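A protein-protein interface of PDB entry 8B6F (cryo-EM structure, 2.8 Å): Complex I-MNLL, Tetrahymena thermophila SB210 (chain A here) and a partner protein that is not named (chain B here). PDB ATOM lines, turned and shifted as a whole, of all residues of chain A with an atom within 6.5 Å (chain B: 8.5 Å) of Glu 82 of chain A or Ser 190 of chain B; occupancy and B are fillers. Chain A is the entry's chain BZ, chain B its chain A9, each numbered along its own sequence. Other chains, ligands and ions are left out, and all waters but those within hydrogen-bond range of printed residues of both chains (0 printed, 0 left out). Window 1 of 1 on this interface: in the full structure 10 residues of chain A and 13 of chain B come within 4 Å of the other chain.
Of the 14 printed residues of chain A, 8 touch a printed residue of chain B.
Among the printed residues, 18 pairs touch across the chains.
Among the printed residues, no Asp or Glu carboxylate lies within 4 Å of a Lys or Arg side-chain nitrogen of the other chain.
The side-chain carboxylate of Glu 83 of chain A lies within hydrogen-bond range of the backbone NH of Gly 81 of chain A (3.3 Å).
The backbone carbonyl oxygen (O) of Ser 190 of chain B sits at hydrogen-bond distance from the side-chain hydroxyl (OG) of Ser 193 of chain B (2.7 Å).
The backbone carbonyl oxygen (O) of Glu 82 of chain A sits at hydrogen-bond distance from the side-chain hydroxyl (OG) of Ser 85 of chain A (2.5 Å).
The backbone NH (N) of Tyr 19 of chain B lies within hydrogen-bond range of the backbone carbonyl oxygen (O) of Val 14 of chain B, at 2.9 Å.
Glu 82 of chain A touches just these residues of chain B: Tyr 13 (3.2 Å), Leu 17 (3.9 Å), Lys 188 (3.6 Å), Glu 189 (3.3 Å) and Ser 190 (3.0 Å).
Gly 81 of chain A touches one residue of chain B.
Printed residues of chain A within 4 Å of Glu 187 of chain B: Lys 79 (3.2 Å).
Printed residues of chain B within 4 Å of Ala 87 of chain A: Tyr 194 (3.6 Å).
Of the printed residues of chain A, Lys 188 of chain B touches Lys 79 and Glu 82.
Of the printed residues of chain A, Gly 192 of chain B touches Tyr 88.
Ser 85 of chain A touches none of the printed residues of chain B.
The nearest residue of chain A that does not touch Ser 190 of chain B is Lys 79 of chain A (4.4 Å).
Among the printed residues, merely in contact across the chains: Lys 74 of chain A with Ser 190 of chain B, Lys 74 of chain A with Ile 191 of chain B, Leu 78 of chain A with Ser 190 of chain B, Lys 79 of chain A with Glu 187 of chain B, Lys 79 of chain A with Lys 188 of chain B, Lys 79 of chain A with Glu 189 of chain B, Ile 80 of chain A with Tyr 19 of chain B, Gly 81 of chain A with Leu 17 of chain B, Glu 82 of chain A with Leu 17 of chain B, Glu 82 of chain A with Lys 188 of chain B, Glu 82 of chain A with Glu 189 of chain B, Ala 87 of chain A with Tyr 194 of chain B, Tyr 88 of chain A with Ile 191 of chain B, Tyr 88 of chain A with Gly 192 of chain B and Tyr 88 of chain A with Ser 193 of chain B.
The side-chain hydroxyl (OG) of Ser 190 of chain B lies within hydrogen-bond range of the side-chain hydroxyl (OH) of Tyr 88 of chain A, at 2.8 Å.
OE1 of Glu 82 of chain A lies close to N of Ser 190 of chain B (3.3 Å).
The side-chain carboxylate of Glu 82 of chain A lies close to the side-chain hydroxyl of Tyr 13 of chain B (3.3 Å).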
ATOM      1  N   LYS A  74     -18.005   2.418   7.246  1.00  0.00           N
ATOM      2  CA  LYS A  74     -17.274   3.680   7.183  1.00  0.00           C
ATOM      3  C   LYS A  74     -16.084   3.582   6.239  1.00  0.00           C
ATOM      4  O   LYS A  74     -15.839   4.494   5.442  1.00  0.00           O
ATOM      5  CB  LYS A  74     -16.814   4.077   8.586  1.00  0.00           C
ATOM      6  CG  LYS A  74     -16.073   5.404   8.665  1.00  0.00           C
ATOM      7  CD  LYS A  74     -16.987   6.574   8.355  1.00  0.00           C
ATOM      8  CE  LYS A  74     -16.277   7.899   8.583  1.00  0.00           C
ATOM      9  NZ  LYS A  74     -17.186   9.059   8.375  1.00  0.00           N
ATOM     10  N   SER A  77     -17.237   3.594   2.733  1.00  0.00           N
ATOM     11  CA  SER A  77     -17.811   4.878   2.350  1.00  0.00           C
ATOM     12  C   SER A  77     -16.754   5.929   2.039  1.00  0.00           C
ATOM     13  O   SER A  77     -17.104   7.002   1.539  1.00  0.00           O
ATOM     14  CB  SER A  77     -18.722   5.398   3.464  1.00  0.00           C
ATOM     15  OG  SER A  77     -19.767   4.483   3.740  1.00  0.00           O
ATOM     16  N   LEU A  78     -15.486   5.650   2.323  1.00  0.00           N
ATOM     17  CA  LEU A  78     -14.431   6.619   2.066  1.00  0.00           C
ATOM     18  C   LEU A  78     -14.413   7.014   0.597  1.00  0.00           C
ATOM     19  O   LEU A  78     -14.541   6.171  -0.294  1.00  0.00           O
ATOM     20  CB  LEU A  78     -13.073   6.039   2.468  1.00  0.00           C
ATOM     21  CG  LEU A  78     -12.915   5.656   3.939  1.00  0.00           C
ATOM     22  CD1 LEU A  78     -11.588   4.954   4.161  1.00  0.00           C
ATOM     23  CD2 LEU A  78     -13.027   6.877   4.831  1.00  0.00           C
ATOM     24  N   LYS A  79     -14.253   8.309   0.348  1.00  0.00           N
ATOM     25  CA  LYS A  79     -14.180   8.801  -1.016  1.00  0.00           C
ATOM     26  C   LYS A  79     -12.912   8.291  -1.692  1.00  0.00           C
ATOM     27  O   LYS A  79     -11.924   7.942  -1.043  1.00  0.00           O
ATOM     28  CB  LYS A  79     -14.216  10.329  -1.042  1.00  0.00           C
ATOM     29  CG  LYS A  79     -15.618  10.923  -0.960  1.00  0.00           C
ATOM     30  CD  LYS A  79     -16.309  10.578   0.350  1.00  0.00           C
ATOM     31  CE  LYS A  79     -17.688  11.216   0.422  1.00  0.00           C
ATOM     32  NZ  LYS A  79     -18.388  10.889   1.694  1.00  0.00           N
ATOM     33  N   ILE A  80     -12.956   8.244  -3.025  1.00  0.00           N
ATOM     34  CA  ILE A  80     -11.824   7.740  -3.791  1.00  0.00           C
ATOM     35  C   ILE A  80     -10.576   8.527  -3.425  1.00  0.00           C
ATOM     36  O   ILE A  80     -10.577   9.764  -3.416  1.00  0.00           O
ATOM     37  CB  ILE A  80     -12.127   7.816  -5.295  1.00  0.00           C
ATOM     38  CG1 ILE A  80     -11.012   7.156  -6.112  1.00  0.00           C
ATOM     39  CG2 ILE A  80     -12.319   9.262  -5.739  1.00  0.00           C
ATOM     40  CD1 ILE A  80     -10.891   5.667  -5.900  1.00  0.00           C
ATOM     41  N   GLY A  81      -9.502   7.806  -3.102  1.00  0.00           N
ATOM     42  CA  GLY A  81      -8.239   8.405  -2.749  1.00  0.00           C
ATOM     43  C   GLY A  81      -7.986   8.510  -1.260  1.00  0.00           C
ATOM     44  O   GLY A  81      -6.832   8.685  -0.856  1.00  0.00           O
ATOM     45  N   GLU A  82      -9.027   8.410  -0.438  1.00  0.00           N
ATOM     46  CA  GLU A  82      -8.879   8.524   1.005  1.00  0.00           C
ATOM     47  C   GLU A  82      -8.532   7.207   1.683  1.00  0.00           C
ATOM     48  O   GLU A  82      -8.127   7.221   2.850  1.00  0.00           O
ATOM     49  CB  GLU A  82     -10.176   9.056   1.617  1.00  0.00           C
ATOM     50  CG  GLU A  82     -10.577  10.423   1.112  1.00  0.00           C
ATOM     51  CD  GLU A  82     -11.797  10.963   1.823  1.00  0.00           C
ATOM     52  OE1 GLU A  82     -12.240  10.335   2.805  1.00  0.00           O
ATOM     53  OE2 GLU A  82     -12.311  12.019   1.404  1.00  0.00           O
ATOM     54  N   GLU A  83      -8.672   6.077   0.990  1.00  0.00           N
ATOM     55  CA  GLU A  83      -8.409   4.792   1.625  1.00  0.00           C
ATOM     56  C   GLU A  83      -6.921   4.544   1.835  1.00  0.00           C
ATOM     57  O   GLU A  83      -6.561   3.711   2.671  1.00  0.00           O
ATOM     58  CB  GLU A  83      -9.018   3.649   0.809  1.00  0.00           C
ATOM     59  CG  GLU A  83      -8.825   3.753  -0.694  1.00  0.00           C
ATOM     60  CD  GLU A  83      -9.949   4.509  -1.382  1.00  0.00           C
ATOM     61  OE1 GLU A  83     -10.821   5.053  -0.675  1.00  0.00           O
ATOM     62  OE2 GLU A  83      -9.961   4.562  -2.629  1.00  0.00           O
ATOM     63  N   LEU A  84      -6.055   5.245   1.104  1.00  0.00           N
ATOM     64  CA  LEU A  84      -4.614   5.153   1.297  1.00  0.00           C
ATOM     65  C   LEU A  84      -4.038   6.405   1.945  1.00  0.00           C
ATOM     66  O   LEU A  84      -2.814   6.543   2.027  1.00  0.00           O
ATOM     67  CB  LEU A  84      -3.914   4.883  -0.038  1.00  0.00           C
ATOM     68  CG  LEU A  84      -4.105   3.491  -0.649  1.00  0.00           C
ATOM     69  CD1 LEU A  84      -3.387   3.399  -1.984  1.00  0.00           C
ATOM     70  CD2 LEU A  84      -3.622   2.392   0.287  1.00  0.00           C
ATOM     71  N   SER A  85      -4.890   7.316   2.404  1.00  0.00           N
ATOM     72  CA  SER A  85      -4.421   8.514   3.079  1.00  0.00           C
ATOM     73  C   SER A  85      -3.890   8.163   4.467  1.00  0.00           C
ATOM     74  O   SER A  85      -4.166   7.097   5.020  1.00  0.00           O
ATOM     75  CB  SER A  85      -5.544   9.545   3.184  1.00  0.00           C
ATOM     76  OG  SER A  85      -6.656   9.025   3.891  1.00  0.00           O
ATOM     77  N   ASP A  86      -3.112   9.088   5.031  1.00  0.00           N
ATOM     78  CA  ASP A  86      -2.504   8.857   6.335  1.00  0.00           C
ATOM     79  C   ASP A  86      -3.535   8.717   7.447  1.00  0.00           C
ATOM     80  O   ASP A  86      -3.225   8.136   8.492  1.00  0.00           O
ATOM     81  CB  ASP A  86      -1.535   9.993   6.667  1.00  0.00           C
ATOM     82  CG  ASP A  86      -0.365  10.062   5.703  1.00  0.00           C
ATOM     83  OD1 ASP A  86      -0.283   9.198   4.806  1.00  0.00           O
ATOM     84  OD2 ASP A  86       0.471  10.978   5.841  1.00  0.00           O
ATOM     85  N   ALA A  87      -4.749   9.227   7.252  1.00  0.00           N
ATOM     86  CA  ALA A  87      -5.777   9.146   8.281  1.00  0.00           C
ATOM     87  C   ALA A  87      -6.562   7.844   8.249  1.00  0.00           C
ATOM     88  O   ALA A  87      -7.248   7.530   9.227  1.00  0.00           O
ATOM     89  CB  ALA A  87      -6.753  10.317   8.145  1.00  0.00           C
ATOM     90  N   TYR A  88      -6.487   7.083   7.155  1.00  0.00           N
ATOM     91  CA  TYR A  88      -7.235   5.842   7.028  1.00  0.00           C
ATOM     92  C   TYR A  88      -6.408   4.679   6.502  1.00  0.00           C
ATOM     93  O   TYR A  88      -6.923   3.556   6.459  1.00  0.00           O
ATOM     94  CB  TYR A  88      -8.442   6.038   6.096  1.00  0.00           C
ATOM     95  CG  TYR A  88      -9.426   7.080   6.571  1.00  0.00           C
ATOM     96  CD1 TYR A  88     -10.269   6.831   7.645  1.00  0.00           C
ATOM     97  CD2 TYR A  88      -9.525   8.310   5.933  1.00  0.00           C
ATOM     98  CE1 TYR A  88     -11.174   7.779   8.077  1.00  0.00           C
ATOM     99  CE2 TYR A  88     -10.427   9.265   6.358  1.00  0.00           C
ATOM    100  CZ  TYR A  88     -11.248   8.993   7.430  1.00  0.00           C
ATOM    101  OH  TYR A  88     -12.149   9.937   7.859  1.00  0.00           O
ATOM    102  N   ARG A  89      -5.153   4.900   6.111  1.00  0.00           N
ATOM    103  CA  ARG A  89      -4.370   3.842   5.478  1.00  0.00           C
ATOM    104  C   ARG A  89      -4.159   2.668   6.426  1.00  0.00           C
ATOM    105  O   ARG A  89      -4.334   1.506   6.044  1.00  0.00           O
ATOM    106  CB  ARG A  89      -3.030   4.401   5.003  1.00  0.00           C
ATOM    107  CG  ARG A  89      -2.070   3.346   4.489  1.00  0.00           C
ATOM    108  CD  ARG A  89      -0.894   3.976   3.766  1.00  0.00           C
ATOM    109  NE  ARG A  89      -0.338   5.095   4.517  1.00  0.00           N
ATOM    110  CZ  ARG A  89       0.543   4.980   5.501  1.00  0.00           C
ATOM    111  NH1 ARG A  89       0.992   3.800   5.892  1.00  0.00           N
ATOM    112  NH2 ARG A  89       0.979   6.077   6.111  1.00  0.00           N
ATOM    113  N   TYR B  13      -7.319  19.629   0.128  1.00  0.00           N
ATOM    114  CA  TYR B  13      -7.578  18.197   0.239  1.00  0.00           C
ATOM    115  C   TYR B  13      -7.406  17.495  -1.103  1.00  0.00           C
ATOM    116  O   TYR B  13      -6.816  16.410  -1.170  1.00  0.00           O
ATOM    117  CB  TYR B  13      -8.979  17.965   0.796  1.00  0.00           C
ATOM    118  CG  TYR B  13      -9.160  16.598   1.404  1.00  0.00           C
ATOM    119  CD1 TYR B  13      -8.486  16.250   2.566  1.00  0.00           C
ATOM    120  CD2 TYR B  13     -10.017  15.666   0.837  1.00  0.00           C
ATOM    121  CE1 TYR B  13      -8.643  15.014   3.139  1.00  0.00           C
ATOM    122  CE2 TYR B  13     -10.183  14.419   1.408  1.00  0.00           C
ATOM    123  CZ  TYR B  13      -9.491  14.102   2.561  1.00  0.00           C
ATOM    124  OH  TYR B  13      -9.637  12.871   3.150  1.00  0.00           O
ATOM    125  N   VAL B  14      -7.928  18.081  -2.181  1.00  0.00           N
ATOM    126  CA  VAL B  14      -7.778  17.462  -3.494  1.00  0.00           C
ATOM    127  C   VAL B  14      -6.310  17.437  -3.902  1.00  0.00           C
ATOM    128  O   VAL B  14      -5.846  16.487  -4.541  1.00  0.00           O
ATOM    129  CB  VAL B  14      -8.646  18.184  -4.542  1.00  0.00           C
ATOM    130  CG1 VAL B  14     -10.112  18.125  -4.152  1.00  0.00           C
ATOM    131  CG2 VAL B  14      -8.196  19.620  -4.726  1.00  0.00           C
ATOM    132  N   VAL B  16      -3.607  17.254  -1.845  1.00  0.00           N
ATOM    133  CA  VAL B  16      -2.878  16.235  -1.095  1.00  0.00           C
ATOM    134  C   VAL B  16      -3.256  14.843  -1.586  1.00  0.00           C
ATOM    135  O   VAL B  16      -2.414  13.939  -1.635  1.00  0.00           O
ATOM    136  CB  VAL B  16      -3.126  16.390   0.416  1.00  0.00           C
ATOM    137  CG1 VAL B  16      -2.602  17.727   0.906  1.00  0.00           C
ATOM    138  CG2 VAL B  16      -4.599  16.251   0.736  1.00  0.00           C
ATOM    139  N   LEU B  17      -4.524  14.640  -1.948  1.00  0.00           N
ATOM    140  CA  LEU B  17      -4.950  13.345  -2.460  1.00  0.00           C
ATOM    141  C   LEU B  17      -4.496  13.093  -3.891  1.00  0.00           C
ATOM    142  O   LEU B  17      -4.436  11.932  -4.308  1.00  0.00           O
ATOM    143  CB  LEU B  17      -6.474  13.218  -2.400  1.00  0.00           C
ATOM    144  CG  LEU B  17      -7.139  13.103  -1.027  1.00  0.00           C
ATOM    145  CD1 LEU B  17      -8.638  12.950  -1.203  1.00  0.00           C
ATOM    146  CD2 LEU B  17      -6.577  11.952  -0.210  1.00  0.00           C
ATOM    147  N   TYR B  19      -6.331  14.215  -6.332  1.00  0.00           N
ATOM    148  CA  TYR B  19      -7.564  14.256  -7.098  1.00  0.00           C
ATOM    149  C   TYR B  19      -7.524  15.429  -8.076  1.00  0.00           C
ATOM    150  O   TYR B  19      -7.048  16.513  -7.722  1.00  0.00           O
ATOM    151  CB  TYR B  19      -8.756  14.397  -6.148  1.00  0.00           C
ATOM    152  CG  TYR B  19     -10.111  14.167  -6.775  1.00  0.00           C
ATOM    153  CD1 TYR B  19     -10.658  12.894  -6.842  1.00  0.00           C
ATOM    154  CD2 TYR B  19     -10.853  15.226  -7.274  1.00  0.00           C
ATOM    155  CE1 TYR B  19     -11.899  12.680  -7.404  1.00  0.00           C
ATOM    156  CE2 TYR B  19     -12.097  15.024  -7.838  1.00  0.00           C
ATOM    157  CZ  TYR B  19     -12.614  13.748  -7.900  1.00  0.00           C
ATOM    158  OH  TYR B  19     -13.852  13.539  -8.459  1.00  0.00           O
ATOM    159  N   GLU B 187     -21.175  15.488  -0.173  1.00  0.00           N
ATOM    160  CA  GLU B 187     -19.901  15.366   0.523  1.00  0.00           C
ATOM    161  C   GLU B 187     -18.852  14.729  -0.375  1.00  0.00           C
ATOM    162  O   GLU B 187     -19.102  13.704  -1.017  1.00  0.00           O
ATOM    163  CB  GLU B 187     -20.064  14.537   1.797  1.00  0.00           C
ATOM    164  CG  GLU B 187     -20.602  15.313   2.984  1.00  0.00           C
ATOM    165  CD  GLU B 187     -22.047  15.720   2.811  1.00  0.00           C
ATOM    166  OE1 GLU B 187     -22.688  15.241   1.853  1.00  0.00           O
ATOM    167  OE2 GLU B 187     -22.542  16.517   3.634  1.00  0.00           O
ATOM    168  N   LYS B 188     -17.670  15.346  -0.417  1.00  0.00           N
ATOM    169  CA  LYS B 188     -16.507  14.787  -1.096  1.00  0.00           C
ATOM    170  C   LYS B 188     -15.355  14.549  -0.127  1.00  0.00           C
ATOM    171  O   LYS B 188     -14.214  14.357  -0.556  1.00  0.00           O
ATOM    172  CB  LYS B 188     -16.064  15.696  -2.243  1.00  0.00           C
ATOM    173  CG  LYS B 188     -17.065  15.764  -3.385  1.00  0.00           C
ATOM    174  CD  LYS B 188     -16.503  16.525  -4.575  1.00  0.00           C
ATOM    175  CE  LYS B 188     -17.467  16.493  -5.752  1.00  0.00           C
ATOM    176  NZ  LYS B 188     -16.933  17.228  -6.932  1.00  0.00           N
ATOM    177  N   GLU B 189     -15.636  14.569   1.174  1.00  0.00           N
ATOM    178  CA  GLU B 189     -14.646  14.282   2.199  1.00  0.00           C
ATOM    179  C   GLU B 189     -15.290  13.426   3.278  1.00  0.00           C
ATOM    180  O   GLU B 189     -16.479  13.566   3.573  1.00  0.00           O
ATOM    181  CB  GLU B 189     -14.088  15.562   2.828  1.00  0.00           C
ATOM    182  CG  GLU B 189     -13.501  16.536   1.828  1.00  0.00           C
ATOM    183  CD  GLU B 189     -13.044  17.824   2.479  1.00  0.00           C
ATOM    184  OE1 GLU B 189     -13.338  18.027   3.675  1.00  0.00           O
ATOM    185  OE2 GLU B 189     -12.390  18.636   1.795  1.00  0.00           O
ATOM    186  N   SER B 190     -14.492  12.541   3.865  1.00  0.00           N
ATOM    187  CA  SER B 190     -14.962  11.725   4.973  1.00  0.00           C
ATOM    188  C   SER B 190     -15.002  12.558   6.248  1.00  0.00           C
ATOM    189  O   SER B 190     -14.107  13.366   6.506  1.00  0.00           O
ATOM    190  CB  SER B 190     -14.052  10.511   5.161  1.00  0.00           C
ATOM    191  OG  SER B 190     -14.483   9.708   6.243  1.00  0.00           O
ATOM    192  N   ILE B 191     -16.053  12.362   7.044  1.00  0.00           N
ATOM    193  CA  ILE B 191     -16.197  13.115   8.283  1.00  0.00           C
ATOM    194  C   ILE B 191     -15.090  12.709   9.245  1.00  0.00           C
ATOM    195  O   ILE B 191     -14.885  11.520   9.520  1.00  0.00           O
ATOM    196  CB  ILE B 191     -17.589  12.890   8.896  1.00  0.00           C
ATOM    197  CG1 ILE B 191     -18.657  13.692   8.142  1.00  0.00           C
ATOM    198  CG2 ILE B 191     -17.616  13.281  10.372  1.00  0.00           C
ATOM    199  CD1 ILE B 191     -18.928  13.222   6.727  1.00  0.00           C
ATOM    200  N   GLY B 192     -14.373  13.700   9.765  1.00  0.00           N
ATOM    201  CA  GLY B 192     -13.242  13.457  10.630  1.00  0.00           C
ATOM    202  C   GLY B 192     -11.920  13.294   9.917  1.00  0.00           C
ATOM    203  O   GLY B 192     -10.895  13.115  10.585  1.00  0.00           O
ATOM    204  N   SER B 193     -11.905  13.353   8.588  1.00  0.00           N
ATOM    205  CA  SER B 193     -10.664  13.201   7.848  1.00  0.00           C
ATOM    206  C   SER B 193      -9.753  14.402   8.075  1.00  0.00           C
ATOM    207  O   SER B 193     -10.196  15.499   8.429  1.00  0.00           O
ATOM    208  CB  SER B 193     -10.947  13.036   6.356  1.00  0.00           C
ATOM    209  OG  SER B 193     -11.638  14.158   5.840  1.00  0.00           O
ATOM    210  N   TYR B 194      -8.460  14.183   7.869  1.00  0.00           N
ATOM    211  CA  TYR B 194      -7.460  15.221   8.073  1.00  0.00           C
ATOM    212  C   TYR B 194      -6.226  14.863   7.256  1.00  0.00           C
ATOM    213  O   TYR B 194      -6.186  13.842   6.566  1.00  0.00           O
ATOM    214  CB  TYR B 194      -7.126  15.376   9.559  1.00  0.00           C
ATOM    215  CG  TYR B 194      -6.510  14.143  10.179  1.00  0.00           C
ATOM    216  CD1 TYR B 194      -5.135  13.951  10.169  1.00  0.00           C
ATOM    217  CD2 TYR B 194      -7.302  13.175  10.777  1.00  0.00           C
ATOM    218  CE1 TYR B 194      -4.567  12.827  10.732  1.00  0.00           C
ATOM    219  CE2 TYR B 194      -6.743  12.047  11.343  1.00  0.00           C
ATOM    220  CZ  TYR B 194      -5.375  11.880  11.318  1.00  0.00           C
ATOM    221  OH  TYR B 194      -4.811  10.760  11.882  1.00  0.00           O
